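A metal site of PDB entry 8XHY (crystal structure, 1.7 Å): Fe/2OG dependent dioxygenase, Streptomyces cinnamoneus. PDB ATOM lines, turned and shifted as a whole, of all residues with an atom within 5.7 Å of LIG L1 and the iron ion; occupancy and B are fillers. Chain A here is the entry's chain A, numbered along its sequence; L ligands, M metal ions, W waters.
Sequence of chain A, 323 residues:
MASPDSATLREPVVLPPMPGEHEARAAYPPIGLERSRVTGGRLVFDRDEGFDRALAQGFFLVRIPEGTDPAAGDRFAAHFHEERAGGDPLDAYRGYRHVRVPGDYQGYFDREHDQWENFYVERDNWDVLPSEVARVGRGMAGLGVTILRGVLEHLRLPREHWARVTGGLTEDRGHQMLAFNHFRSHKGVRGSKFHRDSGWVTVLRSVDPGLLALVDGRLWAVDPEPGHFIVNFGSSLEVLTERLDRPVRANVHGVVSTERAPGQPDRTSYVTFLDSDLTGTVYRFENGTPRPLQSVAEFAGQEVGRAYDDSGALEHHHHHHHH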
ATOM      1  N   TRP A 116      -5.780  21.321 -11.851  1.00  0.00           N
ATOM      2  CA  TRP A 116      -6.955  20.546 -12.231  1.00  0.00           C
ATOM      3  C   TRP A 116      -7.788  21.281 -13.263  1.00  0.00           C
ATOM      4  O   TRP A 116      -7.813  22.507 -13.321  1.00  0.00           O
ATOM      5  CB  TRP A 116      -7.824  20.146 -11.038  1.00  0.00           C
ATOM      6  CG  TRP A 116      -8.406  21.201 -10.138  1.00  0.00           C
ATOM      7  CD1 TRP A 116      -8.355  22.564 -10.267  1.00  0.00           C
ATOM      8  CD2 TRP A 116      -9.113  20.931  -8.927  1.00  0.00           C
ATOM      9  NE1 TRP A 116      -8.989  23.160  -9.190  1.00  0.00           N
ATOM     10  CE2 TRP A 116      -9.478  22.172  -8.369  1.00  0.00           C
ATOM     11  CE3 TRP A 116      -9.486  19.753  -8.272  1.00  0.00           C
ATOM     12  CZ2 TRP A 116     -10.206  22.268  -7.165  1.00  0.00           C
ATOM     13  CZ3 TRP A 116     -10.217  19.835  -7.082  1.00  0.00           C
ATOM     14  CH2 TRP A 116     -10.568  21.084  -6.551  1.00  0.00           C
ATOM     15  N   TYR A 120     -18.127  18.881 -13.960  1.00  0.00           N
ATOM     16  CA  TYR A 120     -19.057  18.840 -12.844  1.00  0.00           C
ATOM     17  C   TYR A 120     -20.468  18.609 -13.361  1.00  0.00           C
ATOM     18  O   TYR A 120     -20.926  19.337 -14.243  1.00  0.00           O
ATOM     19  CB  TYR A 120     -19.045  20.167 -12.058  1.00  0.00           C
ATOM     20  CG  TYR A 120     -17.807  20.479 -11.206  1.00  0.00           C
ATOM     21  CD1 TYR A 120     -16.806  19.544 -10.981  1.00  0.00           C
ATOM     22  CD2 TYR A 120     -17.676  21.712 -10.613  1.00  0.00           C
ATOM     23  CE1 TYR A 120     -15.704  19.828 -10.198  1.00  0.00           C
ATOM     24  CE2 TYR A 120     -16.554  22.025  -9.806  1.00  0.00           C
ATOM     25  CZ  TYR A 120     -15.588  21.077  -9.603  1.00  0.00           C
ATOM     26  OH  TYR A 120     -14.495  21.381  -8.796  1.00  0.00           O
ATOM     27  N   ALA A 179     -18.336  14.963  -9.706  1.00  0.00           N
ATOM     28  CA  ALA A 179     -17.311  15.923 -10.074  1.00  0.00           C
ATOM     29  C   ALA A 179     -16.055  15.174 -10.446  1.00  0.00           C
ATOM     30  O   ALA A 179     -15.521  14.429  -9.608  1.00  0.00           O
ATOM     31  CB  ALA A 179     -17.041  16.876  -8.894  1.00  0.00           C
ATOM     32  N   ASN A 181     -12.038  15.229 -11.683  1.00  0.00           N
ATOM     33  CA  ASN A 181     -10.851  16.084 -11.635  1.00  0.00           C
ATOM     34  C   ASN A 181      -9.718  15.450 -12.414  1.00  0.00           C
ATOM     35  O   ASN A 181      -9.365  14.291 -12.154  1.00  0.00           O
ATOM     36  CB  ASN A 181     -10.348  16.282 -10.202  1.00  0.00           C
ATOM     37  CG  ASN A 181     -11.388  16.862  -9.289  1.00  0.00           C
ATOM     38  OD1 ASN A 181     -12.114  17.801  -9.657  1.00  0.00           O
ATOM     39  ND2 ASN A 181     -11.531  16.273  -8.089  1.00  0.00           N
ATOM     40  N   PHE A 183      -5.745  16.349 -12.967  1.00  0.00           N
ATOM     41  CA  PHE A 183      -4.674  17.245 -12.572  1.00  0.00           C
ATOM     42  C   PHE A 183      -3.675  17.305 -13.724  1.00  0.00           C
ATOM     43  O   PHE A 183      -3.008  16.306 -14.034  1.00  0.00           O
ATOM     44  CB  PHE A 183      -4.047  16.780 -11.259  1.00  0.00           C
ATOM     45  CG  PHE A 183      -5.016  16.873 -10.125  1.00  0.00           C
ATOM     46  CD1 PHE A 183      -5.851  15.802  -9.833  1.00  0.00           C
ATOM     47  CD2 PHE A 183      -5.123  18.024  -9.378  1.00  0.00           C
ATOM     48  CE1 PHE A 183      -6.793  15.850  -8.819  1.00  0.00           C
ATOM     49  CE2 PHE A 183      -6.070  18.115  -8.349  1.00  0.00           C
ATOM     50  CZ  PHE A 183      -6.901  16.993  -8.049  1.00  0.00           C
ATOM     51  N   SER A 192      -4.609  22.004  -6.697  1.00  0.00           N
ATOM     52  CA  SER A 192      -5.773  22.859  -6.498  1.00  0.00           C
ATOM     53  C   SER A 192      -5.356  23.985  -5.544  1.00  0.00           C
ATOM     54  O   SER A 192      -4.341  23.898  -4.870  1.00  0.00           O
ATOM     55  CB  SER A 192      -6.936  22.091  -5.859  1.00  0.00           C
ATOM     56  OG  SER A 192      -6.642  21.784  -4.499  1.00  0.00           O
ATOM     57  N   HIS A 195      -8.784  24.862  -0.139  1.00  0.00           N
ATOM     58  CA  HIS A 195     -10.194  25.219  -0.141  1.00  0.00           C
ATOM     59  C   HIS A 195     -10.942  24.393   0.908  1.00  0.00           C
ATOM     60  O   HIS A 195     -10.468  23.349   1.356  1.00  0.00           O
ATOM     61  CB  HIS A 195     -10.832  24.974  -1.537  1.00  0.00           C
ATOM     62  CG  HIS A 195     -10.833  23.529  -1.944  1.00  0.00           C
ATOM     63  ND1 HIS A 195      -9.758  22.899  -2.540  1.00  0.00           N
ATOM     64  CD2 HIS A 195     -11.795  22.586  -1.812  1.00  0.00           C
ATOM     65  CE1 HIS A 195     -10.059  21.640  -2.776  1.00  0.00           C
ATOM     66  NE2 HIS A 195     -11.296  21.426  -2.352  1.00  0.00           N
ATOM     67  N   ARG A 196     -12.103  24.904   1.313  1.00  0.00           N
ATOM     68  CA  ARG A 196     -13.125  24.075   1.923  1.00  0.00           C
ATOM     69  C   ARG A 196     -14.169  23.732   0.868  1.00  0.00           C
ATOM     70  O   ARG A 196     -14.482  24.550  -0.009  1.00  0.00           O
ATOM     71  CB  ARG A 196     -13.817  24.774   3.097  1.00  0.00           C
ATOM     72  CG  ARG A 196     -12.839  24.974   4.256  1.00  0.00           C
ATOM     73  CD  ARG A 196     -13.540  25.701   5.431  1.00  0.00           C
ATOM     74  NE  ARG A 196     -13.417  27.115   5.204  1.00  0.00           N
ATOM     75  CZ  ARG A 196     -12.951  28.005   6.083  1.00  0.00           C
ATOM     76  NH1 ARG A 196     -12.613  27.643   7.329  1.00  0.00           N
ATOM     77  NH2 ARG A 196     -12.889  29.269   5.718  1.00  0.00           N
ATOM     78  N   ASP A 197     -14.674  22.516   0.926  1.00  0.00           N
ATOM     79  CA  ASP A 197     -15.809  22.171   0.069  1.00  0.00           C
ATOM     80  C   ASP A 197     -17.016  22.906   0.632  1.00  0.00           C
ATOM     81  O   ASP A 197     -17.077  23.168   1.827  1.00  0.00           O
ATOM     82  CB  ASP A 197     -16.083  20.667   0.061  1.00  0.00           C
ATOM     83  CG  ASP A 197     -14.926  19.831  -0.517  1.00  0.00           C
ATOM     84  OD1 ASP A 197     -14.052  20.419  -1.194  1.00  0.00           O
ATOM     85  OD2 ASP A 197     -14.920  18.589  -0.322  1.00  0.00           O
ATOM     86  N   THR A 202     -18.700  15.253   1.488  1.00  0.00           N
ATOM     87  CA  THR A 202     -18.032  14.948   0.221  1.00  0.00           C
ATOM     88  C   THR A 202     -17.522  13.512   0.263  1.00  0.00           C
ATOM     89  O   THR A 202     -16.860  13.114   1.224  1.00  0.00           O
ATOM     90  CB  THR A 202     -16.843  15.896  -0.014  1.00  0.00           C
ATOM     91  OG1 THR A 202     -17.304  17.256  -0.005  1.00  0.00           O
ATOM     92  CG2 THR A 202     -16.127  15.607  -1.396  1.00  0.00           C
ATOM     93  N   LEU A 204     -15.059  10.964  -1.700  1.00  0.00           N
ATOM     94  CA  LEU A 204     -13.941  11.181  -2.621  1.00  0.00           C
ATOM     95  C   LEU A 204     -13.330   9.851  -3.029  1.00  0.00           C
ATOM     96  O   LEU A 204     -12.857   9.091  -2.176  1.00  0.00           O
ATOM     97  CB  LEU A 204     -12.864  12.069  -1.972  1.00  0.00           C
ATOM     98  CG  LEU A 204     -11.432  12.067  -2.554  1.00  0.00           C
ATOM     99  CD1 LEU A 204     -11.328  12.672  -3.936  1.00  0.00           C
ATOM    100  CD2 LEU A 204     -10.455  12.795  -1.587  1.00  0.00           C
ATOM    101  N   SER A 206     -10.219   8.437  -4.827  1.00  0.00           N
ATOM    102  CA  SER A 206      -8.861   8.698  -5.284  1.00  0.00           C
ATOM    103  C   SER A 206      -8.026   7.474  -4.970  1.00  0.00           C
ATOM    104  O   SER A 206      -8.398   6.647  -4.124  1.00  0.00           O
ATOM    105  CB  SER A 206      -8.267   9.941  -4.594  1.00  0.00           C
ATOM    106  OG  SER A 206      -8.277   9.728  -3.200  1.00  0.00           O
ATOM    107  N   GLY A 210      -1.319  12.949  -2.571  1.00  0.00           N
ATOM    108  CA  GLY A 210      -1.227  14.327  -3.016  1.00  0.00           C
ATOM    109  C   GLY A 210      -2.232  15.248  -2.357  1.00  0.00           C
ATOM    110  O   GLY A 210      -2.128  16.484  -2.427  1.00  0.00           O
ATOM    111  N   LEU A 211      -3.208  14.667  -1.648  1.00  0.00           N
ATOM    112  CA  LEU A 211      -4.150  15.520  -0.935  1.00  0.00           C
ATOM    113  C   LEU A 211      -3.507  15.933   0.404  1.00  0.00           C
ATOM    114  O   LEU A 211      -2.981  15.074   1.114  1.00  0.00           O
ATOM    115  CB  LEU A 211      -5.490  14.801  -0.724  1.00  0.00           C
ATOM    116  CG  LEU A 211      -6.527  15.542   0.126  1.00  0.00           C
ATOM    117  CD1 LEU A 211      -6.957  16.936  -0.442  1.00  0.00           C
ATOM    118  CD2 LEU A 211      -7.741  14.601   0.302  1.00  0.00           C
ATOM    119  N   ASN A 232     -15.052  13.826   3.721  1.00  0.00           N
ATOM    120  CA  ASN A 232     -14.853  15.025   4.520  1.00  0.00           C
ATOM    121  C   ASN A 232     -16.149  15.819   4.551  1.00  0.00           C
ATOM    122  O   ASN A 232     -17.171  15.448   3.955  1.00  0.00           O
ATOM    123  CB  ASN A 232     -13.671  15.877   4.037  1.00  0.00           C
ATOM    124  CG  ASN A 232     -13.837  16.357   2.615  1.00  0.00           C
ATOM    125  OD1 ASN A 232     -13.398  15.696   1.694  1.00  0.00           O
ATOM    126  ND2 ASN A 232     -14.408  17.539   2.441  1.00  0.00           N
ATOM    127  N   HIS A 253      -8.221  22.025   2.597  1.00  0.00           N
ATOM    128  CA  HIS A 253      -7.432  20.956   1.982  1.00  0.00           C
ATOM    129  C   HIS A 253      -7.134  21.342   0.546  1.00  0.00           C
ATOM    130  O   HIS A 253      -7.815  22.188  -0.041  1.00  0.00           O
ATOM    131  CB  HIS A 253      -8.189  19.603   2.065  1.00  0.00           C
ATOM    132  CG  HIS A 253      -9.506  19.614   1.350  1.00  0.00           C
ATOM    133  ND1 HIS A 253     -10.643  20.199   1.877  1.00  0.00           N
ATOM    134  CD2 HIS A 253      -9.843  19.209   0.105  1.00  0.00           C
ATOM    135  CE1 HIS A 253     -11.634  20.090   1.020  1.00  0.00           C
ATOM    136  NE2 HIS A 253     -11.171  19.483  -0.064  1.00  0.00           N
ATOM    137  N   GLY A 254      -6.128  20.678  -0.042  1.00  0.00           N
ATOM    138  CA  GLY A 254      -5.822  20.970  -1.442  1.00  0.00           C
ATOM    139  C   GLY A 254      -4.820  19.959  -1.921  1.00  0.00           C
ATOM    140  O   GLY A 254      -4.251  19.196  -1.145  1.00  0.00           O
ATOM    141  N   VAL A 255      -4.606  19.946  -3.233  1.00  0.00           N
ATOM    142  CA  VAL A 255      -3.760  18.934  -3.848  1.00  0.00           C
ATOM    143  C   VAL A 255      -2.430  19.549  -4.240  1.00  0.00           C
ATOM    144  O   VAL A 255      -2.373  20.666  -4.801  1.00  0.00           O
ATOM    145  CB  VAL A 255      -4.460  18.300  -5.064  1.00  0.00           C
ATOM    146  CG1 VAL A 255      -3.522  17.304  -5.790  1.00  0.00           C
ATOM    147  CG2 VAL A 255      -5.676  17.564  -4.575  1.00  0.00           C
ATOM    148  N   ARG A 267      -2.454  12.353 -12.315  1.00  0.00           N
ATOM    149  CA  ARG A 267      -3.358  12.128 -11.190  1.00  0.00           C
ATOM    150  C   ARG A 267      -4.774  12.527 -11.568  1.00  0.00           C
ATOM    151  O   ARG A 267      -4.991  13.523 -12.258  1.00  0.00           O
ATOM    152  CB  ARG A 267      -2.888  12.946  -9.978  1.00  0.00           C
ATOM    153  CG  ARG A 267      -3.663  12.582  -8.684  1.00  0.00           C
ATOM    154  CD  ARG A 267      -3.072  13.382  -7.511  1.00  0.00           C
ATOM    155  NE  ARG A 267      -3.621  12.934  -6.214  1.00  0.00           N
ATOM    156  CZ  ARG A 267      -4.821  13.288  -5.741  1.00  0.00           C
ATOM    157  NH1 ARG A 267      -5.614  14.116  -6.414  1.00  0.00           N
ATOM    158  NH2 ARG A 267      -5.228  12.780  -4.575  1.00  0.00           N
ATOM    159  N   THR A 268      -5.747  11.739 -11.141  1.00  0.00           N
ATOM    160  CA  THR A 268      -7.143  12.115 -11.297  1.00  0.00           C
ATOM    161  C   THR A 268      -7.833  11.810  -9.981  1.00  0.00           C
ATOM    162  O   THR A 268      -7.314  11.097  -9.114  1.00  0.00           O
ATOM    163  CB  THR A 268      -7.844  11.384 -12.456  1.00  0.00           C
ATOM    164  OG1 THR A 268      -7.938   9.985 -12.149  1.00  0.00           O
ATOM    165  CG2 THR A 268      -7.048  11.550 -13.785  1.00  0.00           C
ATOM    166  N   SER A 269      -9.031  12.361  -9.827  1.00  0.00           N
ATOM    167  CA  SER A 269      -9.895  11.937  -8.726  1.00  0.00           C
ATOM    168  C   SER A 269     -11.313  12.305  -9.114  1.00  0.00           C
ATOM    169  O   SER A 269     -11.511  13.077 -10.059  1.00  0.00           O
ATOM    170  CB  SER A 269      -9.536  12.596  -7.411  1.00  0.00           C
ATOM    171  OG  SER A 269      -9.615  14.029  -7.465  1.00  0.00           O
ATOM    172  N   VAL A 271     -15.474  12.921  -7.108  1.00  0.00           N
ATOM    173  CA  VAL A 271     -16.184  13.071  -5.833  1.00  0.00           C
ATOM    174  C   VAL A 271     -17.660  13.219  -6.128  1.00  0.00           C
ATOM    175  O   VAL A 271     -18.056  13.578  -7.241  1.00  0.00           O
ATOM    176  CB  VAL A 271     -15.753  14.304  -4.992  1.00  0.00           C
ATOM    177  CG1 VAL A 271     -14.275  14.342  -4.786  1.00  0.00           C
ATOM    178  CG2 VAL A 271     -16.230  15.563  -5.644  1.00  0.00           C
ATOM    179  N   PHE A 273     -20.239  15.818  -4.377  1.00  0.00           N
ATOM    180  CA  PHE A 273     -20.515  16.922  -3.455  1.00  0.00           C
ATOM    181  C   PHE A 273     -22.012  16.941  -3.150  1.00  0.00           C
ATOM    182  O   PHE A 273     -22.837  16.936  -4.080  1.00  0.00           O
ATOM    183  CB  PHE A 273     -20.141  18.270  -4.079  1.00  0.00           C
ATOM    184  CG  PHE A 273     -18.677  18.454  -4.411  1.00  0.00           C
ATOM    185  CD1 PHE A 273     -17.695  18.469  -3.397  1.00  0.00           C
ATOM    186  CD2 PHE A 273     -18.289  18.749  -5.731  1.00  0.00           C
ATOM    187  CE1 PHE A 273     -16.364  18.710  -3.698  1.00  0.00           C
ATOM    188  CE2 PHE A 273     -16.913  18.998  -6.050  1.00  0.00           C
ATOM    189  CZ  PHE A 273     -15.960  18.995  -5.012  1.00  0.00           C
HETATM  190  C1  LIG L   1     -12.138  18.327  -4.508  1.00  0.00           C
HETATM  191  O1  LIG L   1     -12.542  17.835  -5.620  1.00  0.00           O
HETATM  192  O2  LIG L   1     -12.797  19.221  -3.932  1.00  0.00           O
HETATM  193  C2  LIG L   1     -10.915  17.836  -3.846  1.00  0.00           C
HETATM  194  O3  LIG L   1     -10.527  18.321  -2.767  1.00  0.00           O
HETATM  195  C3  LIG L   1     -10.127  16.720  -4.500  1.00  0.00           C
HETATM  196  C4  LIG L   1      -9.158  16.032  -3.548  1.00  0.00           C
HETATM  197  C5  LIG L   1      -8.245  15.041  -4.260  1.00  0.00           C
HETATM  198  O4  LIG L   1      -8.178  15.026  -5.492  1.00  0.00           O
HETATM  199  O5  LIG L   1      -7.550  14.243  -3.564  1.00  0.00           O
HETATM  200  C1  LG2 L   2     -20.294  24.535  -5.749  1.00  0.00           C
HETATM  201  C2  LG2 L   2     -22.491  23.401  -6.057  1.00  0.00           C
HETATM  202  C3  LG2 L   2     -16.565  22.467  -4.909  1.00  0.00           C
HETATM  203  C4  LG2 L   2     -17.732  22.439  -3.952  1.00  0.00           C
HETATM  204  C5  LG2 L   2     -19.333  23.304  -5.791  1.00  0.00           C
HETATM  205  C6  LG2 L   2     -18.076  23.636  -6.616  1.00  0.00           C
HETATM  206  C7  LG2 L   2     -15.260  22.882  -4.193  1.00  0.00           C
HETATM  207  C8  LG2 L   2     -13.967  22.330  -4.992  1.00  0.00           C
HETATM  208  C9  LG2 L   2     -15.221  24.392  -4.078  1.00  0.00           C
HETATM  209  C10 LG2 L   2     -16.413  25.155  -3.301  1.00  0.00           C
HETATM  210  C11 LG2 L   2     -21.635  24.170  -5.016  1.00  0.00           C
HETATM  211  C12 LG2 L   2     -22.351  25.453  -4.548  1.00  0.00           C
HETATM  212  N1  LG2 L   2     -16.831  23.241  -6.144  1.00  0.00           N
HETATM  213  N2  LG2 L   2     -19.001  22.822  -4.406  1.00  0.00           N
HETATM  214  O1  LG2 L   2     -18.143  24.233  -7.674  1.00  0.00           O
HETATM  215  O2  LG2 L   2     -17.572  22.047  -2.793  1.00  0.00           O
HETATM  216 FE    FE M   1     -12.163  19.506  -1.954  1.00  0.00          FE
HETATM  217  O   HOH W   1     -13.691  19.015  -7.756  1.00  0.00           O
HETATM  218  O   HOH W   2      -7.065  11.900  -2.169  1.00  0.00           O
HETATM  219  O   HOH W   3     -13.000  17.570  -1.531  1.00  0.00           O
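O1 of LIG L1 is in hydrogen-bond range of ND2 of Asn 181 (3.1 Å).
An oxygen (O4) of LIG L1 lies within hydrogen-bond range of the side-chain hydroxyl (OG) of Ser 269, 2.6 Å away.
The guanidinium group (NH1) of Arg 267 is in salt-bridge range of an oxygen (O4) of LIG L1.
Residues that only touch LIG L1: Trp 116 (3.4 Å), Phe 183 (3.5 Å), Leu 204 (3.8 Å), Leu 211 (3.6 Å), Val 255 (3.6 Å), Val 271 (3.99 Å) and Phe 273 (3.3 Å).
Hydrophobic or aromatic side chains that line LIG L1: Trp 116, Phe 183, His 195, Leu 204, Leu 211, His 253, Val 255, Val 271 and Phe 273.
Of the 23 residues printed, 13 come within 4 Å of LIG L1.
The nearest printed residue that does not touch LIG L1 is Ser 206 (4.5 Å).
Within 4 Å of the iron ion: His 195, Asp 197 and His 253.
The backbone carbonyl oxygen of Ser 269 is in hydrogen-bond range of the backbone NH of Asn 181.
N of Val 255 lies within hydrogen-bond range of OG of Ser 192 (3.0 Å).
The backbone NH of Ala 179 lies within hydrogen-bond range of the backbone carbonyl oxygen of Val 271 (2.8 Å).
The backbone carbonyl oxygen (O) of Arg 267 lies within hydrogen-bond range of the backbone NH (N) of Phe 183, 3.0 Å away.
The side-chain carboxylate (OD2) of Asp 197 is in hydrogen-bond range of the side-chain amide nitrogen (ND2) of Asn 232 (3.0 Å).
OD2 of Asp 197 lies within hydrogen-bond range of OG1 of Thr 202, 2.7 Å away.
Water W1 lies within hydrogen-bond range of O1 of LIG L1, OH of Tyr 120 and OD1 of Asn 181.
Water W2 lies within hydrogen-bond range of the side-chain hydroxyl of Ser 206 (2.7 Å), an oxygen (O5) of LIG L1 (2.8 Å) and the guanidinium group of Arg 267 (3.2 Å).
The iron ion is bound by O2 of LIG L1 (2.1 Å), NE2 of His 253 (2.1 Å), NE2 of His 195 (2.1 Å), water W3 (2.2 Å), O3 of LIG L1 (2.2 Å) and OD1 of Asp 197 (2.2 Å).
The iron ion has six donor atoms within binding distance.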
